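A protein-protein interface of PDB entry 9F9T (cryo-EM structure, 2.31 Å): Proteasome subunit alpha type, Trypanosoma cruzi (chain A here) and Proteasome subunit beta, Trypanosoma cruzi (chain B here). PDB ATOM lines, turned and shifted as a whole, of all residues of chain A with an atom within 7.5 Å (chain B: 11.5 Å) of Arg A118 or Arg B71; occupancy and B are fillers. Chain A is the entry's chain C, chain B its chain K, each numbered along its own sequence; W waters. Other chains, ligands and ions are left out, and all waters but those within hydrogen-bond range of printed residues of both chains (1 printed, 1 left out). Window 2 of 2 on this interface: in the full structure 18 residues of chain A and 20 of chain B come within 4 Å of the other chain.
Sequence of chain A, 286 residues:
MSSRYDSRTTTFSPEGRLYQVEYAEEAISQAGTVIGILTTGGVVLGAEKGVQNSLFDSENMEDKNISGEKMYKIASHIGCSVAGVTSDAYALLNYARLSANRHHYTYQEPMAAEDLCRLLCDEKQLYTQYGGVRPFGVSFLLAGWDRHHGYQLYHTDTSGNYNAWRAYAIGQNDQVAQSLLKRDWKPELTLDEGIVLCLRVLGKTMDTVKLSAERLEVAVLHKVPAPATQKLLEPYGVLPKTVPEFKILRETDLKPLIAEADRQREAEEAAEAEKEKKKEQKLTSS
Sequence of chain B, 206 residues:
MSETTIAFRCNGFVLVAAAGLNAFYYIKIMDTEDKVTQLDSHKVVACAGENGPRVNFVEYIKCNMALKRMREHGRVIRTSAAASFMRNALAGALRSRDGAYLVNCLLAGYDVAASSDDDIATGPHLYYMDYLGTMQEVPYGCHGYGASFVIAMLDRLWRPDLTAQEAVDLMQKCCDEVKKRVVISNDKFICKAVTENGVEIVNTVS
NE2 of His B73 lies within hydrogen-bond range of OE1 of Glu A114 (3.4 Å).
The guanidinium group (NH1) of Arg A118 lies within hydrogen-bond range of a ring nitrogen (NE2) of His B73 (3.4 Å).
OD1 of Asp A115 lies close to O of Arg B71, at 2.8 Å.
NH1 of Arg A118 lies within salt-bridge range of OE1 of Glu A114, 3.2 Å away.
The side-chain carboxylate (OE1) of Glu A114 sits at hydrogen-bond distance from the side-chain hydroxyl (OH) of Tyr A162.
Among the printed residues, pairs that only touch across the chains: Ala A112 with Glu B72 (3.3 Å), Arg A118 with Arg B71 (3.6 Å) and Asp A115 with Glu B72 (3.98 Å).
Of chain B, only Arg B71 and His B73 come within 4 Å of Arg A118.
Of chain A, only Asp A115 and Arg A118 come within 4 Å of Arg B71.
Glu A114 touches just one residue of chain B: His B73 (3.4 Å).
No residue of chain B comes within 4 Å of Leu A116.
No residue of chain B comes within 4 Å of Cys A117.
No residue of chain B comes within 4 Å of Leu A119.
Leu A120 touches none of the printed residues of chain B.
Cys A121 touches none of the printed residues of chain B.
No residue of chain B comes within 4 Å of Asp A122.
Printed residues of chain A within 4 Å of His B73: Glu A114 and Arg A118.
Printed residues of chain B within 4 Å of Asp A115: Arg B71 and Glu B72.
Of the printed residues of chain A, Glu B72 touches Ala A112 and Asp A115.
Of the printed residues of chain B, Ala A112 touches Glu B72.
Met B70 touches none of the printed residues of chain A.
The nearest residue of chain A that does not touch Arg B71 is Glu A114 (6.9 Å).
The nearest printed residue of chain A that does not touch Glu B72 is Arg A118 (4.7 Å).
Of the 19 printed residues of chain A, 4 touch a printed residue of chain B.
Printed residues of chain A that touch a printed residue of chain B: Ala A112, Glu A114, Asp A115 and Arg A118.
Along chain A the printed residues that touch a printed residue of chain B span positions 112 to 118.
Water W1 lies within hydrogen-bond range of OE1 of Glu B72 and N of Ala A112.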
ATOM      1  N   TYR A  95       8.949  -0.252  10.746  1.00  0.00           N
ATOM      2  CA  TYR A  95       7.647  -0.739  11.154  1.00  0.00           C
ATOM      3  C   TYR A  95       7.423  -2.142  10.595  1.00  0.00           C
ATOM      4  O   TYR A  95       7.016  -3.046  11.324  1.00  0.00           O
ATOM      5  CB  TYR A  95       6.590   0.288  10.738  1.00  0.00           C
ATOM      6  CG  TYR A  95       5.231  -0.179  11.228  1.00  0.00           C
ATOM      7  CD1 TYR A  95       4.899  -0.107  12.581  1.00  0.00           C
ATOM      8  CD2 TYR A  95       4.346  -0.827  10.374  1.00  0.00           C
ATOM      9  CE1 TYR A  95       3.703  -0.624  13.053  1.00  0.00           C
ATOM     10  CE2 TYR A  95       3.158  -1.362  10.840  1.00  0.00           C
ATOM     11  CZ  TYR A  95       2.828  -1.254  12.177  1.00  0.00           C
ATOM     12  OH  TYR A  95       1.638  -1.775  12.607  1.00  0.00           O
ATOM     13  N   MET A 111       5.694 -14.537   7.712  1.00  0.00           N
ATOM     14  CA  MET A 111       4.450 -13.836   7.454  1.00  0.00           C
ATOM     15  C   MET A 111       4.173 -13.869   5.955  1.00  0.00           C
ATOM     16  O   MET A 111       5.101 -13.816   5.155  1.00  0.00           O
ATOM     17  CB  MET A 111       4.608 -12.403   7.943  1.00  0.00           C
ATOM     18  CG  MET A 111       3.412 -11.496   7.750  1.00  0.00           C
ATOM     19  SD  MET A 111       3.728  -9.975   8.680  1.00  0.00           S
ATOM     20  CE  MET A 111       2.102  -9.675   9.336  1.00  0.00           C
ATOM     21  N   ALA A 112       2.919 -14.051   5.566  1.00  0.00           N
ATOM     22  CA  ALA A 112       2.553 -13.952   4.161  1.00  0.00           C
ATOM     23  C   ALA A 112       2.704 -12.524   3.637  1.00  0.00           C
ATOM     24  O   ALA A 112       2.407 -11.565   4.333  1.00  0.00           O
ATOM     25  CB  ALA A 112       1.131 -14.381   4.026  1.00  0.00           C
ATOM     26  N   ALA A 113       3.150 -12.376   2.386  1.00  0.00           N
ATOM     27  CA  ALA A 113       3.535 -11.060   1.880  1.00  0.00           C
ATOM     28  C   ALA A 113       2.335 -10.128   1.758  1.00  0.00           C
ATOM     29  O   ALA A 113       2.476  -8.923   1.942  1.00  0.00           O
ATOM     30  CB  ALA A 113       4.258 -11.217   0.573  1.00  0.00           C
ATOM     31  N   GLU A 114       1.132 -10.673   1.546  1.00  0.00           N
ATOM     32  CA  GLU A 114      -0.050  -9.824   1.502  1.00  0.00           C
ATOM     33  C   GLU A 114      -0.450  -9.331   2.892  1.00  0.00           C
ATOM     34  O   GLU A 114      -0.815  -8.179   3.050  1.00  0.00           O
ATOM     35  CB  GLU A 114      -1.256 -10.502   0.857  1.00  0.00           C
ATOM     36  CG  GLU A 114      -2.298  -9.451   0.459  1.00  0.00           C
ATOM     37  CD  GLU A 114      -3.659  -9.925  -0.041  1.00  0.00           C
ATOM     38  OE1 GLU A 114      -4.677  -9.299   0.374  1.00  0.00           O
ATOM     39  OE2 GLU A 114      -3.704 -10.892  -0.865  1.00  0.00           O
ATOM     40  N   ASP A 115      -0.374 -10.204   3.889  1.00  0.00           N
ATOM     41  CA  ASP A 115      -0.577  -9.860   5.282  1.00  0.00           C
ATOM     42  C   ASP A 115       0.388  -8.731   5.682  1.00  0.00           C
ATOM     43  O   ASP A 115      -0.012  -7.826   6.389  1.00  0.00           O
ATOM     44  CB  ASP A 115      -0.402 -11.132   6.132  1.00  0.00           C
ATOM     45  CG  ASP A 115      -1.366 -11.407   7.285  1.00  0.00           C
ATOM     46  OD1 ASP A 115      -2.541 -11.797   6.976  1.00  0.00           O
ATOM     47  OD2 ASP A 115      -0.929 -11.296   8.490  1.00  0.00           O
ATOM     48  N   LEU A 116       1.661  -8.784   5.246  1.00  0.00           N
ATOM     49  CA  LEU A 116       2.659  -7.786   5.625  1.00  0.00           C
ATOM     50  C   LEU A 116       2.284  -6.442   5.027  1.00  0.00           C
ATOM     51  O   LEU A 116       2.340  -5.415   5.675  1.00  0.00           O
ATOM     52  CB  LEU A 116       4.082  -8.172   5.171  1.00  0.00           C
ATOM     53  CG  LEU A 116       5.213  -7.197   5.568  1.00  0.00           C
ATOM     54  CD1 LEU A 116       5.382  -6.096   4.543  1.00  0.00           C
ATOM     55  CD2 LEU A 116       4.994  -6.550   6.936  1.00  0.00           C
ATOM     56  N   CYS A 117       1.842  -6.524   3.792  1.00  0.00           N
ATOM     57  CA  CYS A 117       1.495  -5.376   3.000  1.00  0.00           C
ATOM     58  C   CYS A 117       0.290  -4.623   3.561  1.00  0.00           C
ATOM     59  O   CYS A 117       0.286  -3.391   3.590  1.00  0.00           O
ATOM     60  CB  CYS A 117       1.234  -5.899   1.601  1.00  0.00           C
ATOM     61  SG  CYS A 117       0.978  -4.516   0.493  1.00  0.00           S
ATOM     62  N   ARG A 118      -0.727  -5.383   3.982  1.00  0.00           N
ATOM     63  CA  ARG A 118      -1.855  -4.830   4.700  1.00  0.00           C
ATOM     64  C   ARG A 118      -1.420  -4.096   5.963  1.00  0.00           C
ATOM     65  O   ARG A 118      -1.966  -3.042   6.239  1.00  0.00           O
ATOM     66  CB  ARG A 118      -2.867  -5.908   5.107  1.00  0.00           C
ATOM     67  CG  ARG A 118      -4.001  -6.067   4.108  1.00  0.00           C
ATOM     68  CD  ARG A 118      -4.493  -7.480   3.838  1.00  0.00           C
ATOM     69  NE  ARG A 118      -5.677  -7.866   4.592  1.00  0.00           N
ATOM     70  CZ  ARG A 118      -6.516  -8.835   4.227  1.00  0.00           C
ATOM     71  NH1 ARG A 118      -6.344  -9.480   3.084  1.00  0.00           N
ATOM     72  NH2 ARG A 118      -7.547  -9.143   4.999  1.00  0.00           N
ATOM     73  N   LEU A 119      -0.529  -4.663   6.793  1.00  0.00           N
ATOM     74  CA  LEU A 119      -0.150  -3.947   8.006  1.00  0.00           C
ATOM     75  C   LEU A 119       0.535  -2.644   7.636  1.00  0.00           C
ATOM     76  O   LEU A 119       0.349  -1.626   8.281  1.00  0.00           O
ATOM     77  CB  LEU A 119       0.762  -4.773   8.913  1.00  0.00           C
ATOM     78  CG  LEU A 119       0.011  -5.764   9.804  1.00  0.00           C
ATOM     79  CD1 LEU A 119       0.964  -6.613  10.642  1.00  0.00           C
ATOM     80  CD2 LEU A 119      -0.990  -5.035  10.697  1.00  0.00           C
ATOM     81  N   LEU A 120       1.294  -2.653   6.564  1.00  0.00           N
ATOM     82  CA  LEU A 120       2.042  -1.474   6.188  1.00  0.00           C
ATOM     83  C   LEU A 120       1.107  -0.334   5.817  1.00  0.00           C
ATOM     84  O   LEU A 120       1.262   0.783   6.272  1.00  0.00           O
ATOM     85  CB  LEU A 120       2.898  -1.909   5.009  1.00  0.00           C
ATOM     86  CG  LEU A 120       3.999  -0.960   4.604  1.00  0.00           C
ATOM     87  CD1 LEU A 120       4.872  -0.674   5.803  1.00  0.00           C
ATOM     88  CD2 LEU A 120       4.809  -1.600   3.498  1.00  0.00           C
ATOM     89  N   CYS A 121       0.109  -0.685   4.996  1.00  0.00           N
ATOM     90  CA  CYS A 121      -0.852   0.233   4.423  1.00  0.00           C
ATOM     91  C   CYS A 121      -1.843   0.747   5.448  1.00  0.00           C
ATOM     92  O   CYS A 121      -2.244   1.903   5.325  1.00  0.00           O
ATOM     93  CB  CYS A 121      -1.616  -0.457   3.322  1.00  0.00           C
ATOM     94  SG  CYS A 121      -0.539  -0.692   1.894  1.00  0.00           S
ATOM     95  N   ASP A 122      -2.200  -0.088   6.437  1.00  0.00           N
ATOM     96  CA  ASP A 122      -2.985   0.351   7.580  1.00  0.00           C
ATOM     97  C   ASP A 122      -2.268   1.414   8.394  1.00  0.00           C
ATOM     98  O   ASP A 122      -2.883   2.377   8.835  1.00  0.00           O
ATOM     99  CB  ASP A 122      -3.294  -0.781   8.563  1.00  0.00           C
ATOM    100  CG  ASP A 122      -4.292  -1.836   8.087  1.00  0.00           C
ATOM    101  OD1 ASP A 122      -4.897  -1.670   6.952  1.00  0.00           O
ATOM    102  OD2 ASP A 122      -4.458  -2.843   8.853  1.00  0.00           O
ATOM    103  N   GLU A 123      -0.966   1.247   8.621  1.00  0.00           N
ATOM    104  CA  GLU A 123      -0.199   2.292   9.286  1.00  0.00           C
ATOM    105  C   GLU A 123      -0.308   3.609   8.503  1.00  0.00           C
ATOM    106  O   GLU A 123      -0.313   4.682   9.105  1.00  0.00           O
ATOM    107  CB  GLU A 123       1.271   1.886   9.494  1.00  0.00           C
ATOM    108  CG  GLU A 123       2.094   2.926  10.277  1.00  0.00           C
ATOM    109  CD  GLU A 123       1.726   3.208  11.744  1.00  0.00           C
ATOM    110  OE1 GLU A 123       2.338   4.114  12.357  1.00  0.00           O
ATOM    111  OE2 GLU A 123       0.847   2.502  12.306  1.00  0.00           O
ATOM    112  N   LYS A 124      -0.323   3.556   7.175  1.00  0.00           N
ATOM    113  CA  LYS A 124      -0.323   4.779   6.394  1.00  0.00           C
ATOM    114  C   LYS A 124      -1.683   5.483   6.510  1.00  0.00           C
ATOM    115  O   LYS A 124      -1.738   6.708   6.663  1.00  0.00           O
ATOM    116  CB  LYS A 124      -0.049   4.483   4.917  1.00  0.00           C
ATOM    117  CG  LYS A 124       1.334   3.936   4.613  1.00  0.00           C
ATOM    118  CD  LYS A 124       1.811   4.262   3.221  1.00  0.00           C
ATOM    119  CE  LYS A 124       2.477   3.109   2.510  1.00  0.00           C
ATOM    120  NZ  LYS A 124       2.853   3.551   1.147  1.00  0.00           N
ATOM    121  N   LEU A 142       6.863  -4.249  -2.988  1.00  0.00           N
ATOM    122  CA  LEU A 142       7.229  -5.380  -2.158  1.00  0.00           C
ATOM    123  C   LEU A 142       7.383  -6.582  -3.054  1.00  0.00           C
ATOM    124  O   LEU A 142       6.502  -6.845  -3.856  1.00  0.00           O
ATOM    125  CB  LEU A 142       6.148  -5.671  -1.123  1.00  0.00           C
ATOM    126  CG  LEU A 142       5.717  -4.478  -0.280  1.00  0.00           C
ATOM    127  CD1 LEU A 142       4.480  -4.809   0.519  1.00  0.00           C
ATOM    128  CD2 LEU A 142       6.811  -4.061   0.641  1.00  0.00           C
ATOM    129  N   THR A 156       2.308  -0.002  -3.154  1.00  0.00           N
ATOM    130  CA  THR A 156       1.651   0.572  -2.008  1.00  0.00           C
ATOM    131  C   THR A 156       1.676   2.073  -2.227  1.00  0.00           C
ATOM    132  O   THR A 156       2.696   2.639  -2.563  1.00  0.00           O
ATOM    133  CB  THR A 156       2.332   0.172  -0.686  1.00  0.00           C
ATOM    134  OG1 THR A 156       2.476  -1.203  -0.311  1.00  0.00           O
ATOM    135  CG2 THR A 156       1.502   0.709   0.442  1.00  0.00           C
ATOM    136  N   GLY A 160      -2.691   4.455   1.397  1.00  0.00           N
ATOM    137  CA  GLY A 160      -2.808   3.244   2.164  1.00  0.00           C
ATOM    138  C   GLY A 160      -3.508   2.185   1.345  1.00  0.00           C
ATOM    139  O   GLY A 160      -4.113   1.291   1.919  1.00  0.00           O
ATOM    140  N   TYR A 162      -3.180  -0.725  -1.915  1.00  0.00           N
ATOM    141  CA  TYR A 162      -2.192  -1.602  -2.480  1.00  0.00           C
ATOM    142  C   TYR A 162      -2.803  -2.561  -3.474  1.00  0.00           C
ATOM    143  O   TYR A 162      -3.957  -2.942  -3.346  1.00  0.00           O
ATOM    144  CB  TYR A 162      -1.567  -2.452  -1.371  1.00  0.00           C
ATOM    145  CG  TYR A 162      -2.422  -3.541  -0.755  1.00  0.00           C
ATOM    146  CD1 TYR A 162      -3.118  -3.311   0.423  1.00  0.00           C
ATOM    147  CD2 TYR A 162      -2.487  -4.806  -1.313  1.00  0.00           C
ATOM    148  CE1 TYR A 162      -3.860  -4.308   1.033  1.00  0.00           C
ATOM    149  CE2 TYR A 162      -3.262  -5.811  -0.744  1.00  0.00           C
ATOM    150  CZ  TYR A 162      -3.928  -5.565   0.451  1.00  0.00           C
ATOM    151  OH  TYR A 162      -4.693  -6.549   1.016  1.00  0.00           O
ATOM    152  N   LYS B  62     -10.001 -20.914  19.034  1.00  0.00           N
ATOM    153  CA  LYS B  62     -10.799 -21.046  17.825  1.00  0.00           C
ATOM    154  C   LYS B  62     -11.037 -19.698  17.151  1.00  0.00           C
ATOM    155  O   LYS B  62     -10.971 -19.596  15.941  1.00  0.00           O
ATOM    156  CB  LYS B  62     -12.189 -21.598  18.068  1.00  0.00           C
ATOM    157  CG  LYS B  62     -12.213 -23.083  18.376  1.00  0.00           C
ATOM    158  CD  LYS B  62     -13.557 -23.700  18.841  1.00  0.00           C
ATOM    159  CE  LYS B  62     -14.550 -23.908  17.713  1.00  0.00           C
ATOM    160  NZ  LYS B  62     -13.882 -24.121  16.390  1.00  0.00           N
ATOM    161  N   CYS B  63     -11.333 -18.679  17.929  1.00  0.00           N
ATOM    162  CA  CYS B  63     -11.731 -17.418  17.365  1.00  0.00           C
ATOM    163  C   CYS B  63     -10.524 -16.754  16.731  1.00  0.00           C
ATOM    164  O   CYS B  63     -10.654 -16.325  15.607  1.00  0.00           O
ATOM    165  CB  CYS B  63     -12.528 -16.611  18.408  1.00  0.00           C
ATOM    166  SG  CYS B  63     -14.103 -17.478  18.823  1.00  0.00           S
ATOM    167  N   ASN B  64      -9.359 -16.707  17.385  1.00  0.00           N
ATOM    168  CA  ASN B  64      -8.145 -16.192  16.774  1.00  0.00           C
ATOM    169  C   ASN B  64      -7.702 -16.956  15.525  1.00  0.00           C
ATOM    170  O   ASN B  64      -7.103 -16.357  14.655  1.00  0.00           O
ATOM    171  CB  ASN B  64      -6.990 -16.149  17.753  1.00  0.00           C
ATOM    172  CG  ASN B  64      -7.229 -15.057  18.781  1.00  0.00           C
ATOM    173  OD1 ASN B  64      -6.757 -13.929  18.629  1.00  0.00           O
ATOM    174  ND2 ASN B  64      -8.027 -15.347  19.802  1.00  0.00           N
ATOM    175  N   MET B  65      -7.966 -18.245  15.406  1.00  0.00           N
ATOM    176  CA  MET B  65      -7.606 -18.925  14.189  1.00  0.00           C
ATOM    177  C   MET B  65      -8.584 -18.548  13.092  1.00  0.00           C
ATOM    178  O   MET B  65      -8.231 -18.534  11.933  1.00  0.00           O
ATOM    179  CB  MET B  65      -7.664 -20.457  14.341  1.00  0.00           C
ATOM    180  CG  MET B  65      -6.457 -20.985  15.115  1.00  0.00           C
ATOM    181  SD  MET B  65      -6.552 -22.740  15.343  1.00  0.00           S
ATOM    182  CE  MET B  65      -6.237 -23.211  13.634  1.00  0.00           C
ATOM    183  N   ALA B  66      -9.845 -18.397  13.461  1.00  0.00           N
ATOM    184  CA  ALA B  66     -10.873 -18.064  12.511  1.00  0.00           C
ATOM    185  C   ALA B  66     -10.610 -16.674  11.936  1.00  0.00           C
ATOM    186  O   ALA B  66     -10.734 -16.442  10.734  1.00  0.00           O
ATOM    187  CB  ALA B  66     -12.222 -18.171  13.168  1.00  0.00           C
ATOM    188  N   LEU B  67     -10.097 -15.803  12.774  1.00  0.00           N
ATOM    189  CA  LEU B  67      -9.795 -14.451  12.377  1.00  0.00           C
ATOM    190  C   LEU B  67      -8.561 -14.458  11.506  1.00  0.00           C
ATOM    191  O   LEU B  67      -8.400 -13.579  10.699  1.00  0.00           O
ATOM    192  CB  LEU B  67      -9.639 -13.624  13.648  1.00  0.00           C
ATOM    193  CG  LEU B  67      -9.618 -12.116  13.437  1.00  0.00           C
ATOM    194  CD1 LEU B  67     -11.003 -11.629  13.072  1.00  0.00           C
ATOM    195  CD2 LEU B  67      -9.105 -11.400  14.674  1.00  0.00           C
ATOM    196  N   LYS B  68      -7.662 -15.427  11.661  1.00  0.00           N
ATOM    197  CA  LYS B  68      -6.467 -15.497  10.827  1.00  0.00           C
ATOM    198  C   LYS B  68      -6.824 -16.064   9.455  1.00  0.00           C
ATOM    199  O   LYS B  68      -6.078 -15.927   8.504  1.00  0.00           O
ATOM    200  CB  LYS B  68      -5.392 -16.385  11.442  1.00  0.00           C
ATOM    201  CG  LYS B  68      -3.973 -15.872  11.281  1.00  0.00           C
ATOM    202  CD  LYS B  68      -2.882 -16.940  11.504  1.00  0.00           C
ATOM    203  CE  LYS B  68      -1.647 -16.717  10.646  1.00  0.00           C
ATOM    204  NZ  LYS B  68      -0.887 -17.979  10.439  1.00  0.00           N
ATOM    205  N   ARG B  69      -7.949 -16.718   9.326  1.00  0.00           N
ATOM    206  CA  ARG B  69      -8.245 -17.388   8.083  1.00  0.00           C
ATOM    207  C   ARG B  69      -8.996 -16.446   7.149  1.00  0.00           C
ATOM    208  O   ARG B  69      -8.999 -16.698   5.954  1.00  0.00           O
ATOM    209  CB  ARG B  69      -9.239 -18.539   8.265  1.00  0.00           C
ATOM    210  CG  ARG B  69      -8.658 -19.883   8.625  1.00  0.00           C
ATOM    211  CD  ARG B  69      -9.643 -20.965   8.181  1.00  0.00           C
ATOM    212  NE  ARG B  69     -11.009 -20.784   8.650  1.00  0.00           N
ATOM    213  CZ  ARG B  69     -11.444 -21.050   9.886  1.00  0.00           C
ATOM    214  NH1 ARG B  69     -12.726 -20.887  10.177  1.00  0.00           N
ATOM    215  NH2 ARG B  69     -10.608 -21.482  10.820  1.00  0.00           N
ATOM    216  N   MET B  70      -9.777 -15.488   7.674  1.00  0.00           N
ATOM    217  CA  MET B  70     -10.371 -14.493   6.786  1.00  0.00           C
ATOM    218  C   MET B  70      -9.376 -13.399   6.449  1.00  0.00           C
ATOM    219  O   MET B  70      -9.393 -12.913   5.328  1.00  0.00           O
ATOM    220  CB  MET B  70     -11.638 -13.793   7.262  1.00  0.00           C
ATOM    221  CG  MET B  70     -11.778 -13.611   8.710  1.00  0.00           C
ATOM    222  SD  MET B  70     -13.537 -13.578   9.001  1.00  0.00           S
ATOM    223  CE  MET B  70     -14.071 -15.116   8.249  1.00  0.00           C
ATOM    224  N   ARG B  71      -8.504 -13.041   7.364  1.00  0.00           N
ATOM    225  CA  ARG B  71      -7.441 -12.131   7.009  1.00  0.00           C
ATOM    226  C   ARG B  71      -6.365 -12.899   6.242  1.00  0.00           C
ATOM    227  O   ARG B  71      -5.163 -12.751   6.514  1.00  0.00           O
ATOM    228  CB  ARG B  71      -6.951 -11.455   8.288  1.00  0.00           C
ATOM    229  CG  ARG B  71      -8.103 -10.874   9.098  1.00  0.00           C
ATOM    230  CD  ARG B  71      -7.898  -9.441   9.544  1.00  0.00           C
ATOM    231  NE  ARG B  71      -7.255  -9.355  10.844  1.00  0.00           N
ATOM    232  CZ  ARG B  71      -7.814  -8.798  11.910  1.00  0.00           C
ATOM    233  NH1 ARG B  71      -7.131  -8.700  13.039  1.00  0.00           N
ATOM    234  NH2 ARG B  71      -9.053  -8.333  11.829  1.00  0.00           N
ATOM    235  N   GLU B  72      -6.794 -13.726   5.273  1.00  0.00           N
ATOM    236  CA  GLU B  72      -5.864 -14.590   4.542  1.00  0.00           C
ATOM    237  C   GLU B  72      -6.606 -15.551   3.595  1.00  0.00           C
ATOM    238  O   GLU B  72      -6.083 -16.601   3.230  1.00  0.00           O
ATOM    239  CB  GLU B  72      -4.959 -15.339   5.538  1.00  0.00           C
ATOM    240  CG  GLU B  72      -3.542 -15.571   5.015  1.00  0.00           C
ATOM    241  CD  GLU B  72      -2.440 -15.820   6.036  1.00  0.00           C
ATOM    242  OE1 GLU B  72      -1.280 -16.045   5.590  1.00  0.00           O
ATOM    243  OE2 GLU B  72      -2.721 -15.766   7.263  1.00  0.00           O
ATOM    244  N   HIS B  73      -7.842 -15.185   3.215  1.00  0.00           N
ATOM    245  CA  HIS B  73      -8.610 -15.823   2.152  1.00  0.00           C
ATOM    246  C   HIS B  73      -8.821 -17.316   2.416  1.00  0.00           C
ATOM    247  O   HIS B  73      -8.888 -18.113   1.477  1.00  0.00           O
ATOM    248  CB  HIS B  73      -7.988 -15.448   0.800  1.00  0.00           C
ATOM    249  CG  HIS B  73      -7.630 -13.997   0.829  1.00  0.00           C
ATOM    250  ND1 HIS B  73      -8.562 -13.035   1.169  1.00  0.00           N
ATOM    251  CD2 HIS B  73      -6.460 -13.356   0.689  1.00  0.00           C
ATOM    252  CE1 HIS B  73      -7.979 -11.845   1.191  1.00  0.00           C
ATOM    253  NE2 HIS B  73      -6.704 -12.018   0.898  1.00  0.00           N
ATOM    254  N   GLY B  74      -8.954 -17.685   3.691  1.00  0.00           N
ATOM    255  CA  GLY B  74      -9.362 -19.034   4.060  1.00  0.00           C
ATOM    256  C   GLY B  74      -8.217 -20.041   3.978  1.00  0.00           C
ATOM    257  O   GLY B  74      -8.447 -21.248   3.959  1.00  0.00           O
ATOM    258  N   ARG B  75      -6.985 -19.528   3.970  1.00  0.00           N
ATOM    259  CA  ARG B  75      -5.833 -20.396   3.887  1.00  0.00           C
ATOM    260  C   ARG B  75      -5.646 -21.083   5.236  1.00  0.00           C
ATOM    261  O   ARG B  75      -5.607 -20.419   6.264  1.00  0.00           O
ATOM    262  CB  ARG B  75      -4.607 -19.604   3.421  1.00  0.00           C
ATOM    263  CG  ARG B  75      -3.977 -20.178   2.155  1.00  0.00           C
ATOM    264  CD  ARG B  75      -4.980 -20.395   1.023  1.00  0.00           C
ATOM    265  NE  ARG B  75      -4.375 -20.779  -0.251  1.00  0.00           N
ATOM    266  CZ  ARG B  75      -4.579 -20.162  -1.413  1.00  0.00           C
ATOM    267  NH1 ARG B  75      -5.369 -19.103  -1.481  1.00  0.00           N
ATOM    268  NH2 ARG B  75      -3.987 -20.610  -2.507  1.00  0.00           N
ATOM    269  N   VAL B  76      -5.517 -22.417   5.198  1.00  0.00           N
ATOM    270  CA  VAL B  76      -5.356 -23.236   6.391  1.00  0.00           C
ATOM    271  C   VAL B  76      -3.953 -23.037   6.978  1.00  0.00           C
ATOM    272  O   VAL B  76      -2.910 -23.059   6.334  1.00  0.00           O
ATOM    273  CB  VAL B  76      -5.666 -24.721   6.109  1.00  0.00           C
ATOM    274  CG1 VAL B  76      -5.702 -25.560   7.379  1.00  0.00           C
ATOM    275  CG2 VAL B  76      -6.980 -24.898   5.356  1.00  0.00           C
ATOM    276  N   ILE B  77      -3.945 -22.861   8.277  1.00  0.00           N
ATOM    277  CA  ILE B  77      -2.720 -22.692   9.010  1.00  0.00           C
ATOM    278  C   ILE B  77      -2.118 -24.048   9.333  1.00  0.00           C
ATOM    279  O   ILE B  77      -2.819 -25.040   9.535  1.00  0.00           O
ATOM    280  CB  ILE B  77      -3.055 -21.835  10.226  1.00  0.00           C
ATOM    281  CG1 ILE B  77      -2.082 -22.006  11.382  1.00  0.00           C
ATOM    282  CG2 ILE B  77      -4.489 -22.049  10.640  1.00  0.00           C
ATOM    283  CD1 ILE B  77      -2.379 -21.077  12.566  1.00  0.00           C
ATOM    284  N   PHE B  85       1.129 -20.892  18.446  1.00  0.00           N
ATOM    285  CA  PHE B  85       0.168 -19.915  18.940  1.00  0.00           C
ATOM    286  C   PHE B  85      -0.393 -20.336  20.294  1.00  0.00           C
ATOM    287  O   PHE B  85      -0.553 -19.527  21.178  1.00  0.00           O
ATOM    288  CB  PHE B  85      -0.910 -19.715  17.873  1.00  0.00           C
ATOM    289  CG  PHE B  85      -1.940 -18.692  18.296  1.00  0.00           C
ATOM    290  CD1 PHE B  85      -1.654 -17.342  18.261  1.00  0.00           C
ATOM    291  CD2 PHE B  85      -3.110 -19.073  18.911  1.00  0.00           C
ATOM    292  CE1 PHE B  85      -2.557 -16.392  18.721  1.00  0.00           C
ATOM    293  CE2 PHE B  85      -4.010 -18.120  19.383  1.00  0.00           C
ATOM    294  CZ  PHE B  85      -3.737 -16.782  19.290  1.00  0.00           C
HETATM  295  O   HOH W   1       0.642 -14.678   7.608  1.00  0.00           O
